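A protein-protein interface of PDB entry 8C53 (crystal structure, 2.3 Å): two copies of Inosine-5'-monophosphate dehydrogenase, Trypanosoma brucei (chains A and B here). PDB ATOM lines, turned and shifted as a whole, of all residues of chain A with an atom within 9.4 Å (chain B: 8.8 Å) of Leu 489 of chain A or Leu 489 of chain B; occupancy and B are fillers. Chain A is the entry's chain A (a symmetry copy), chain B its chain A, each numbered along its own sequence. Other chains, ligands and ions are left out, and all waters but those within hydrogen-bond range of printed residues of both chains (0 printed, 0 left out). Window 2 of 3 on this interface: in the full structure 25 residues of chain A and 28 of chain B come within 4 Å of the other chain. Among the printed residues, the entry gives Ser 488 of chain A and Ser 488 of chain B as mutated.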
ATOM      1  N   ASP A  24     -21.034 -12.078   5.972  1.00  0.00           N
ATOM      2  CA  ASP A  24     -20.429 -13.356   6.305  1.00  0.00           C
ATOM      3  C   ASP A  24     -18.903 -13.348   6.280  1.00  0.00           C
ATOM      4  O   ASP A  24     -18.284 -12.471   5.671  1.00  0.00           O
ATOM      5  CB  ASP A  24     -20.936 -14.423   5.328  1.00  0.00           C
ATOM      6  CG  ASP A  24     -20.831 -13.974   3.873  1.00  0.00           C
ATOM      7  OD1 ASP A  24     -20.608 -14.833   2.991  1.00  0.00           O
ATOM      8  OD2 ASP A  24     -20.964 -12.746   3.616  1.00  0.00           O
ATOM      9  N   LEU A  26     -15.172 -13.961   5.397  1.00  0.00           N
ATOM     10  CA  LEU A  26     -14.570 -14.045   4.079  1.00  0.00           C
ATOM     11  C   LEU A  26     -13.173 -14.652   4.129  1.00  0.00           C
ATOM     12  O   LEU A  26     -12.424 -14.439   5.096  1.00  0.00           O
ATOM     13  CB  LEU A  26     -14.475 -12.662   3.437  1.00  0.00           C
ATOM     14  CG  LEU A  26     -15.772 -11.889   3.242  1.00  0.00           C
ATOM     15  CD1 LEU A  26     -15.506 -10.616   2.457  1.00  0.00           C
ATOM     16  CD2 LEU A  26     -16.805 -12.736   2.534  1.00  0.00           C
ATOM     17  N   ASN A  29      -9.753 -15.369  -1.222  1.00  0.00           N
ATOM     18  CA  ASN A  29     -10.231 -15.493  -2.589  1.00  0.00           C
ATOM     19  C   ASN A  29     -11.602 -14.863  -2.791  1.00  0.00           C
ATOM     20  O   ASN A  29     -12.039 -14.730  -3.940  1.00  0.00           O
ATOM     21  CB  ASN A  29     -10.289 -16.963  -3.001  1.00  0.00           C
ATOM     22  CG  ASN A  29      -8.913 -17.563  -3.202  1.00  0.00           C
ATOM     23  OD1 ASN A  29      -8.041 -16.954  -3.830  1.00  0.00           O
ATOM     24  ND2 ASN A  29      -8.704 -18.754  -2.661  1.00  0.00           N
ATOM     25  N   ASP A  30     -12.290 -14.481  -1.721  1.00  0.00           N
ATOM     26  CA  ASP A  30     -13.635 -13.939  -1.856  1.00  0.00           C
ATOM     27  C   ASP A  30     -13.667 -12.516  -2.383  1.00  0.00           C
ATOM     28  O   ASP A  30     -14.745 -12.029  -2.735  1.00  0.00           O
ATOM     29  CB  ASP A  30     -14.355 -13.973  -0.505  1.00  0.00           C
ATOM     30  CG  ASP A  30     -14.983 -15.310  -0.204  1.00  0.00           C
ATOM     31  OD1 ASP A  30     -15.712 -15.847  -1.069  1.00  0.00           O
ATOM     32  OD2 ASP A  30     -14.741 -15.819   0.906  1.00  0.00           O
ATOM     33  N   PHE A  31     -12.532 -11.829  -2.439  1.00  0.00           N
ATOM     34  CA  PHE A  31     -12.525 -10.440  -2.859  1.00  0.00           C
ATOM     35  C   PHE A  31     -11.242 -10.121  -3.614  1.00  0.00           C
ATOM     36  O   PHE A  31     -10.231 -10.825  -3.513  1.00  0.00           O
ATOM     37  CB  PHE A  31     -12.667  -9.497  -1.664  1.00  0.00           C
ATOM     38  CG  PHE A  31     -11.514  -9.562  -0.698  1.00  0.00           C
ATOM     39  CD1 PHE A  31     -11.508 -10.482   0.334  1.00  0.00           C
ATOM     40  CD2 PHE A  31     -10.447  -8.698  -0.816  1.00  0.00           C
ATOM     41  CE1 PHE A  31     -10.463 -10.533   1.228  1.00  0.00           C
ATOM     42  CE2 PHE A  31      -9.396  -8.749   0.077  1.00  0.00           C
ATOM     43  CZ  PHE A  31      -9.408  -9.670   1.098  1.00  0.00           C
ATOM     44  N   ARG A 486     -16.127  -7.611  -3.827  1.00  0.00           N
ATOM     45  CA  ARG A 486     -16.436  -8.998  -3.544  1.00  0.00           C
ATOM     46  C   ARG A 486     -16.602  -9.744  -4.868  1.00  0.00           C
ATOM     47  O   ARG A 486     -17.088  -9.200  -5.862  1.00  0.00           O
ATOM     48  CB  ARG A 486     -17.702  -9.108  -2.705  1.00  0.00           C
ATOM     49  CG  ARG A 486     -18.085 -10.547  -2.406  1.00  0.00           C
ATOM     50  CD  ARG A 486     -18.494 -10.736  -0.962  1.00  0.00           C
ATOM     51  NE  ARG A 486     -18.763 -12.143  -0.682  1.00  0.00           N
ATOM     52  CZ  ARG A 486     -19.514 -12.580   0.317  1.00  0.00           C
ATOM     53  NH1 ARG A 486     -20.114 -11.740   1.151  1.00  0.00           N
ATOM     54  NH2 ARG A 486     -19.666 -13.891   0.485  1.00  0.00           N
ATOM     55  N   ARG A 487     -16.193 -10.992  -4.886  1.00  0.00           N
ATOM     56  CA  ARG A 487     -16.231 -11.801  -6.096  1.00  0.00           C
ATOM     57  C   ARG A 487     -17.253 -12.913  -5.931  1.00  0.00           C
ATOM     58  O   ARG A 487     -17.159 -13.708  -4.994  1.00  0.00           O
ATOM     59  CB  ARG A 487     -14.855 -12.386  -6.399  1.00  0.00           C
ATOM     60  CG  ARG A 487     -13.818 -11.334  -6.670  1.00  0.00           C
ATOM     61  CD  ARG A 487     -12.724 -11.877  -7.547  1.00  0.00           C
ATOM     62  NE  ARG A 487     -11.882 -12.811  -6.820  1.00  0.00           N
ATOM     63  CZ  ARG A 487     -11.011 -13.626  -7.392  1.00  0.00           C
ATOM     64  NH1 ARG A 487     -10.816 -13.616  -8.700  1.00  0.00           N
ATOM     65  NH2 ARG A 487     -10.325 -14.476  -6.634  1.00  0.00           N
ATOM     66  N   SER A 488     -18.222 -12.963  -6.843  1.00  0.00           N
ATOM     67  CA  SER A 488     -19.134 -14.090  -6.878  1.00  0.00           C
ATOM     68  C   SER A 488     -18.327 -15.376  -7.000  1.00  0.00           C
ATOM     69  O   SER A 488     -17.184 -15.381  -7.455  1.00  0.00           O
ATOM     70  CB  SER A 488     -20.105 -13.971  -8.050  1.00  0.00           C
ATOM     71  OG  SER A 488     -19.419 -14.151  -9.283  1.00  0.00           O
ATOM     72  N   LEU A 489     -18.923 -16.475  -6.561  1.00  0.00           N
ATOM     73  CA  LEU A 489     -18.227 -17.754  -6.671  1.00  0.00           C
ATOM     74  C   LEU A 489     -17.844 -18.039  -8.119  1.00  0.00           C
ATOM     75  O   LEU A 489     -16.759 -18.562  -8.393  1.00  0.00           O
ATOM     76  CB  LEU A 489     -19.094 -18.869  -6.110  1.00  0.00           C
ATOM     77  CG  LEU A 489     -18.593 -19.359  -4.756  1.00  0.00           C
ATOM     78  CD1 LEU A 489     -18.783 -18.293  -3.694  1.00  0.00           C
ATOM     79  CD2 LEU A 489     -19.311 -20.648  -4.375  1.00  0.00           C
ATOM     80  N   THR A 490     -18.710 -17.668  -9.059  1.00  0.00           N
ATOM     81  CA  THR A 490     -18.409 -17.874 -10.470  1.00  0.00           C
ATOM     82  C   THR A 490     -17.256 -16.989 -10.924  1.00  0.00           C
ATOM     83  O   THR A 490     -16.429 -17.409 -11.735  1.00  0.00           O
ATOM     84  CB  THR A 490     -19.660 -17.589 -11.311  1.00  0.00           C
ATOM     85  OG1 THR A 490     -20.681 -18.538 -10.972  1.00  0.00           O
ATOM     86  CG2 THR A 490     -19.338 -17.684 -12.796  1.00  0.00           C
ATOM     87  N   ALA A 491     -17.190 -15.760 -10.418  1.00  0.00           N
ATOM     88  CA  ALA A 491     -16.122 -14.844 -10.792  1.00  0.00           C
ATOM     89  C   ALA A 491     -14.762 -15.329 -10.318  1.00  0.00           C
ATOM     90  O   ALA A 491     -13.739 -14.778 -10.744  1.00  0.00           O
ATOM     91  CB  ALA A 491     -16.391 -13.447 -10.222  1.00  0.00           C
ATOM     92  N   GLN A 492     -14.720 -16.326  -9.439  1.00  0.00           N
ATOM     93  CA  GLN A 492     -13.463 -16.859  -8.931  1.00  0.00           C
ATOM     94  C   GLN A 492     -12.876 -17.944  -9.832  1.00  0.00           C
ATOM     95  O   GLN A 492     -12.093 -18.770  -9.358  1.00  0.00           O
ATOM     96  CB  GLN A 492     -13.668 -17.389  -7.510  1.00  0.00           C
ATOM     97  CG  GLN A 492     -14.003 -16.300  -6.495  1.00  0.00           C
ATOM     98  CD  GLN A 492     -14.264 -16.847  -5.100  1.00  0.00           C
ATOM     99  OE1 GLN A 492     -15.183 -16.398  -4.404  1.00  0.00           O
ATOM    100  NE2 GLN A 492     -13.456 -17.812  -4.680  1.00  0.00           N
ATOM    101  N   SER A 493     -13.226 -17.951 -11.116  1.00  0.00           N
ATOM    102  CA  SER A 493     -12.646 -18.888 -12.084  1.00  0.00           C
ATOM    103  C   SER A 493     -12.213 -18.175 -13.370  1.00  0.00           C
ATOM    104  O   SER A 493     -11.033 -17.868 -13.555  1.00  0.00           O
ATOM    105  CB  SER A 493     -13.649 -19.994 -12.407  1.00  0.00           C
ATOM    106  OG  SER A 493     -14.370 -20.368 -11.242  1.00  0.00           O
ATOM    107  N   ASP B  24     -22.062  -7.703  -5.061  1.00  0.00           N
ATOM    108  CA  ASP B  24     -20.767  -8.282  -5.372  1.00  0.00           C
ATOM    109  C   ASP B  24     -20.445  -8.324  -6.863  1.00  0.00           C
ATOM    110  O   ASP B  24     -21.340  -8.238  -7.707  1.00  0.00           O
ATOM    111  CB  ASP B  24     -20.704  -9.706  -4.810  1.00  0.00           C
ATOM    112  CG  ASP B  24     -21.930 -10.533  -5.186  1.00  0.00           C
ATOM    113  OD1 ASP B  24     -21.798 -11.766  -5.361  1.00  0.00           O
ATOM    114  OD2 ASP B  24     -23.034  -9.937  -5.316  1.00  0.00           O
ATOM    115  N   GLY B  25     -19.154  -8.387  -7.181  1.00  0.00           N
ATOM    116  CA  GLY B  25     -18.718  -8.387  -8.569  1.00  0.00           C
ATOM    117  C   GLY B  25     -19.159  -9.643  -9.301  1.00  0.00           C
ATOM    118  O   GLY B  25     -18.963 -10.763  -8.816  1.00  0.00           O
ATOM    119  N   LEU B  26     -19.705  -9.463 -10.500  1.00  0.00           N
ATOM    120  CA  LEU B  26     -20.337 -10.537 -11.245  1.00  0.00           C
ATOM    121  C   LEU B  26     -19.540 -10.915 -12.487  1.00  0.00           C
ATOM    122  O   LEU B  26     -18.920 -10.052 -13.128  1.00  0.00           O
ATOM    123  CB  LEU B  26     -21.748 -10.139 -11.676  1.00  0.00           C
ATOM    124  CG  LEU B  26     -22.737  -9.768 -10.580  1.00  0.00           C
ATOM    125  CD1 LEU B  26     -24.118  -9.554 -11.176  1.00  0.00           C
ATOM    126  CD2 LEU B  26     -22.787 -10.835  -9.511  1.00  0.00           C
ATOM    127  N   SER B  27     -19.551 -12.202 -12.806  1.00  0.00           N
ATOM    128  CA  SER B  27     -19.119 -12.714 -14.093  1.00  0.00           C
ATOM    129  C   SER B  27     -20.329 -12.898 -15.003  1.00  0.00           C
ATOM    130  O   SER B  27     -21.484 -12.768 -14.580  1.00  0.00           O
ATOM    131  CB  SER B  27     -18.382 -14.032 -13.921  1.00  0.00           C
ATOM    132  OG  SER B  27     -17.408 -14.171 -14.946  1.00  0.00           O
ATOM    133  N   ASN B  29     -21.609 -15.534 -16.389  1.00  0.00           N
ATOM    134  CA  ASN B  29     -22.486 -16.651 -16.080  1.00  0.00           C
ATOM    135  C   ASN B  29     -23.391 -16.375 -14.887  1.00  0.00           C
ATOM    136  O   ASN B  29     -24.311 -17.161 -14.636  1.00  0.00           O
ATOM    137  CB  ASN B  29     -21.666 -17.911 -15.807  1.00  0.00           C
ATOM    138  CG  ASN B  29     -21.037 -18.477 -17.063  1.00  0.00           C
ATOM    139  OD1 ASN B  29     -21.689 -18.582 -18.108  1.00  0.00           O
ATOM    140  ND2 ASN B  29     -19.764 -18.833 -16.977  1.00  0.00           N
ATOM    141  N   ASP B  30     -23.155 -15.297 -14.147  1.00  0.00           N
ATOM    142  CA  ASP B  30     -23.945 -15.028 -12.953  1.00  0.00           C
ATOM    143  C   ASP B  30     -25.343 -14.514 -13.254  1.00  0.00           C
ATOM    144  O   ASP B  30     -26.169 -14.450 -12.339  1.00  0.00           O
ATOM    145  CB  ASP B  30     -23.231 -14.002 -12.069  1.00  0.00           C
ATOM    146  CG  ASP B  30     -22.189 -14.621 -11.171  1.00  0.00           C
ATOM    147  OD1 ASP B  30     -22.500 -15.614 -10.476  1.00  0.00           O
ATOM    148  OD2 ASP B  30     -21.057 -14.103 -11.168  1.00  0.00           O
ATOM    149  N   PRO B 336     -14.054  -8.414 -11.451  1.00  0.00           N
ATOM    150  CA  PRO B 336     -14.928  -9.250 -12.283  1.00  0.00           C
ATOM    151  C   PRO B 336     -15.418  -8.499 -13.516  1.00  0.00           C
ATOM    152  O   PRO B 336     -15.840  -7.354 -13.442  1.00  0.00           O
ATOM    153  CB  PRO B 336     -16.082  -9.603 -11.329  1.00  0.00           C
ATOM    154  CG  PRO B 336     -15.435  -9.611  -9.973  1.00  0.00           C
ATOM    155  CD  PRO B 336     -14.415  -8.493 -10.019  1.00  0.00           C
ATOM    156  N   ARG B 486     -30.451 -12.418 -11.949  1.00  0.00           N
ATOM    157  CA  ARG B 486     -29.312 -13.089 -11.356  1.00  0.00           C
ATOM    158  C   ARG B 486     -29.630 -14.579 -11.231  1.00  0.00           C
ATOM    159  O   ARG B 486     -30.769 -14.980 -10.988  1.00  0.00           O
ATOM    160  CB  ARG B 486     -28.986 -12.494  -9.992  1.00  0.00           C
ATOM    161  CG  ARG B 486     -27.815 -13.183  -9.316  1.00  0.00           C
ATOM    162  CD  ARG B 486     -26.857 -12.192  -8.692  1.00  0.00           C
ATOM    163  NE  ARG B 486     -25.695 -12.879  -8.135  1.00  0.00           N
ATOM    164  CZ  ARG B 486     -24.911 -12.382  -7.191  1.00  0.00           C
ATOM    165  NH1 ARG B 486     -25.145 -11.192  -6.652  1.00  0.00           N
ATOM    166  NH2 ARG B 486     -23.864 -13.094  -6.781  1.00  0.00           N
ATOM    167  N   ARG B 487     -28.621 -15.403 -11.402  1.00  0.00           N
ATOM    168  CA  ARG B 487     -28.791 -16.849 -11.375  1.00  0.00           C
ATOM    169  C   ARG B 487     -28.091 -17.419 -10.153  1.00  0.00           C
ATOM    170  O   ARG B 487     -26.888 -17.215  -9.975  1.00  0.00           O
ATOM    171  CB  ARG B 487     -28.237 -17.482 -12.647  1.00  0.00           C
ATOM    172  CG  ARG B 487     -28.956 -17.031 -13.886  1.00  0.00           C
ATOM    173  CD  ARG B 487     -28.859 -18.072 -14.967  1.00  0.00           C
ATOM    174  NE  ARG B 487     -27.517 -18.133 -15.520  1.00  0.00           N
ATOM    175  CZ  ARG B 487     -27.076 -19.111 -16.294  1.00  0.00           C
ATOM    176  NH1 ARG B 487     -27.864 -20.109 -16.657  1.00  0.00           N
ATOM    177  NH2 ARG B 487     -25.812 -19.091 -16.706  1.00  0.00           N
ATOM    178  N   SER B 488     -28.847 -18.132  -9.320  1.00  0.00           N
ATOM    179  CA  SER B 488     -28.237 -18.867  -8.228  1.00  0.00           C
ATOM    180  C   SER B 488     -27.177 -19.802  -8.793  1.00  0.00           C
ATOM    181  O   SER B 488     -27.202 -20.175  -9.966  1.00  0.00           O
ATOM    182  CB  SER B 488     -29.283 -19.669  -7.458  1.00  0.00           C
ATOM    183  OG  SER B 488     -29.772 -20.740  -8.255  1.00  0.00           O
ATOM    184  N   LEU B 489     -26.218 -20.163  -7.953  1.00  0.00           N
ATOM    185  CA  LEU B 489     -25.180 -21.082  -8.410  1.00  0.00           C
ATOM    186  C   LEU B 489     -25.794 -22.380  -8.921  1.00  0.00           C
ATOM    187  O   LEU B 489     -25.334 -22.947  -9.917  1.00  0.00           O
ATOM    188  CB  LEU B 489     -24.193 -21.354  -7.287  1.00  0.00           C
ATOM    189  CG  LEU B 489     -22.863 -20.643  -7.507  1.00  0.00           C
ATOM    190  CD1 LEU B 489     -23.029 -19.141  -7.379  1.00  0.00           C
ATOM    191  CD2 LEU B 489     -21.827 -21.167  -6.520  1.00  0.00           C
ATOM    192  N   THR B 490     -26.858 -22.846  -8.269  1.00  0.00           N
ATOM    193  CA  THR B 490     -27.527 -24.063  -8.710  1.00  0.00           C
ATOM    194  C   THR B 490     -28.210 -23.862 -10.055  1.00  0.00           C
ATOM    195  O   THR B 490     -28.222 -24.769 -10.890  1.00  0.00           O
ATOM    196  CB  THR B 490     -28.550 -24.501  -7.654  1.00  0.00           C
ATOM    197  OG1 THR B 490     -27.860 -24.833  -6.441  1.00  0.00           O
ATOM    198  CG2 THR B 490     -29.342 -25.704  -8.145  1.00  0.00           C
ATOM    199  N   ALA B 491     -28.790 -22.686 -10.279  1.00  0.00           N
ATOM    200  CA  ALA B 491     -29.465 -22.402 -11.538  1.00  0.00           C
ATOM    201  C   ALA B 491     -28.499 -22.377 -12.711  1.00  0.00           C
ATOM    202  O   ALA B 491     -28.947 -22.368 -13.864  1.00  0.00           O
ATOM    203  CB  ALA B 491     -30.204 -21.062 -11.457  1.00  0.00           C
ATOM    204  N   GLN B 492     -27.195 -22.346 -12.453  1.00  0.00           N
ATOM    205  CA  GLN B 492     -26.196 -22.324 -13.512  1.00  0.00           C
ATOM    206  C   GLN B 492     -25.825 -23.722 -14.003  1.00  0.00           C
ATOM    207  O   GLN B 492     -24.736 -23.905 -14.552  1.00  0.00           O
ATOM    208  CB  GLN B 492     -24.953 -21.574 -13.029  1.00  0.00           C
ATOM    209  CG  GLN B 492     -25.197 -20.090 -12.769  1.00  0.00           C
ATOM    210  CD  GLN B 492     -23.971 -19.369 -12.231  1.00  0.00           C
ATOM    211  OE1 GLN B 492     -24.072 -18.531 -11.328  1.00  0.00           O
ATOM    212  NE2 GLN B 492     -22.807 -19.684 -12.786  1.00  0.00           N
ATOM    213  N   SER B 493     -26.709 -24.703 -13.829  1.00  0.00           N
ATOM    214  CA  SER B 493     -26.491 -26.057 -14.348  1.00  0.00           C
ATOM    215  C   SER B 493     -27.734 -26.591 -15.070  1.00  0.00           C
ATOM    216  O   SER B 493     -27.813 -26.556 -16.301  1.00  0.00           O
ATOM    217  CB  SER B 493     -26.099 -26.998 -13.211  1.00  0.00           C
ATOM    218  OG  SER B 493     -25.249 -26.334 -12.286  1.00  0.00           O
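Of the 15 printed residues of chain B, 8 touch a printed residue of chain A.
Among the printed residues, no Asp or Glu carboxylate lies within 4 Å of a Lys or Arg side-chain nitrogen of the other chain.
The side-chain carboxylate (OD1) of Asp 30 of chain B sits close to the side-chain amide oxygen (OE1) of Gln 492 of chain B, 3.4 Å away.
The backbone carbonyl oxygen (O) of Arg 487 of chain B sits close to the side-chain amide oxygen (OE1) of Gln 492 of chain B, 3.4 Å away.
OD2 of Asp 24 of chain B lies within salt-bridge range of NH1 of Arg 486 of chain B (2.8 Å).
NH2 of Arg 487 of chain A lies within hydrogen-bond range of O of Asn 29 of chain A, at 3.2 Å.
The backbone NH (N) of Ser 27 of chain B sits at hydrogen-bond distance from the side-chain carboxylate (OD2) of Asp 30 of chain B, 2.9 Å away.
OE1 of Gln 492 of chain A sits close to O of Arg 487 of chain A (3.4 Å).
Leu 489 of chain A touches just one residue of chain B: Leu 489.
Printed residues of chain B within 4 Å of Thr 490 of chain A: Ser 27 (3.9 Å), Asn 29 (3.8 Å), Asp 30 (3.5 Å) and Gln 492 (3.0 Å).
Gln 492 of chain A touches none of the printed residues of chain B.
Printed residues of chain A within 4 Å of Asp 24 of chain B: Arg 486 (3.6 Å) and Ser 488 (3.8 Å).
Leu 26 of chain B touches none of the printed residues of chain A.
Leu 489 of chain B touches one residue of chain A.
No residue of chain A comes within 4 Å of Thr 490 of chain B.
Printed residues of chain A within 4 Å of Gln 492 of chain B: Thr 490.
The nearest residue of chain B that does not touch Leu 489 of chain A is Asp 30 of chain B (5.4 Å).
The nearest residue of chain A that does not touch Leu 489 of chain B is Thr 490 of chain A (4.3 Å).
The nearest printed residue of chain A that does not touch Pro 336 of chain B is Arg 487 of chain A (4.1 Å).
Ser 488 of chain A touches Asp 30 of chain B, but with the chains exchanged Asp 30 of chain A does not touch Ser 488 of chain B (14.4 Å).
Leu 489 of chain B touches its own counterpart, Leu 489 of chain A.
Thr 490 of chain A touches Asn 29 of chain B, but with the chains exchanged Asn 29 of chain A does not touch Thr 490 of chain B (17.4 Å).
Thr 490 of chain A touches Asp 30 of chain B, but with the chains exchanged Asp 30 of chain A does not touch Thr 490 of chain B (15.0 Å).
Among the printed residues, merely in contact across the chains: Arg 486 of chain A with Asp 24 of chain B, Arg 487 of chain A with Gly 25 of chain B, Ser 488 of chain A with Asp 24 of chain B, Leu 489 of chain A with Leu 489 of chain B, Thr 490 of chain A with Ser 27 of chain B, Thr 490 of chain A with Asn 29 of chain B, Ala 491 of chain A with Gly 25 of chain B, Ala 491 of chain A with Ser 27 of chain B and Ala 491 of chain A with Pro 336 of chain B.
The backbone carbonyl oxygen of Gly 25 of chain B lies within hydrogen-bond range of the backbone NH of Ser 488 of chain A.
OD1 of Asp 30 of chain B lies within hydrogen-bond range of OG1 of Thr 490 of chain A (3.5 Å).
The backbone carbonyl oxygen (O) of Arg 486 of chain A is in hydrogen-bond range of the backbone NH (N) of Gly 25 of chain B, at 2.6 Å.
NE2 of Gln 492 of chain B lies within hydrogen-bond range of OG1 of Thr 490 of chain A (3.0 Å).
The side-chain hydroxyl (OG) of Ser 488 of chain A is in hydrogen-bond range of the side-chain carboxylate (OD2) of Asp 30 of chain B, at 2.5 Å.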
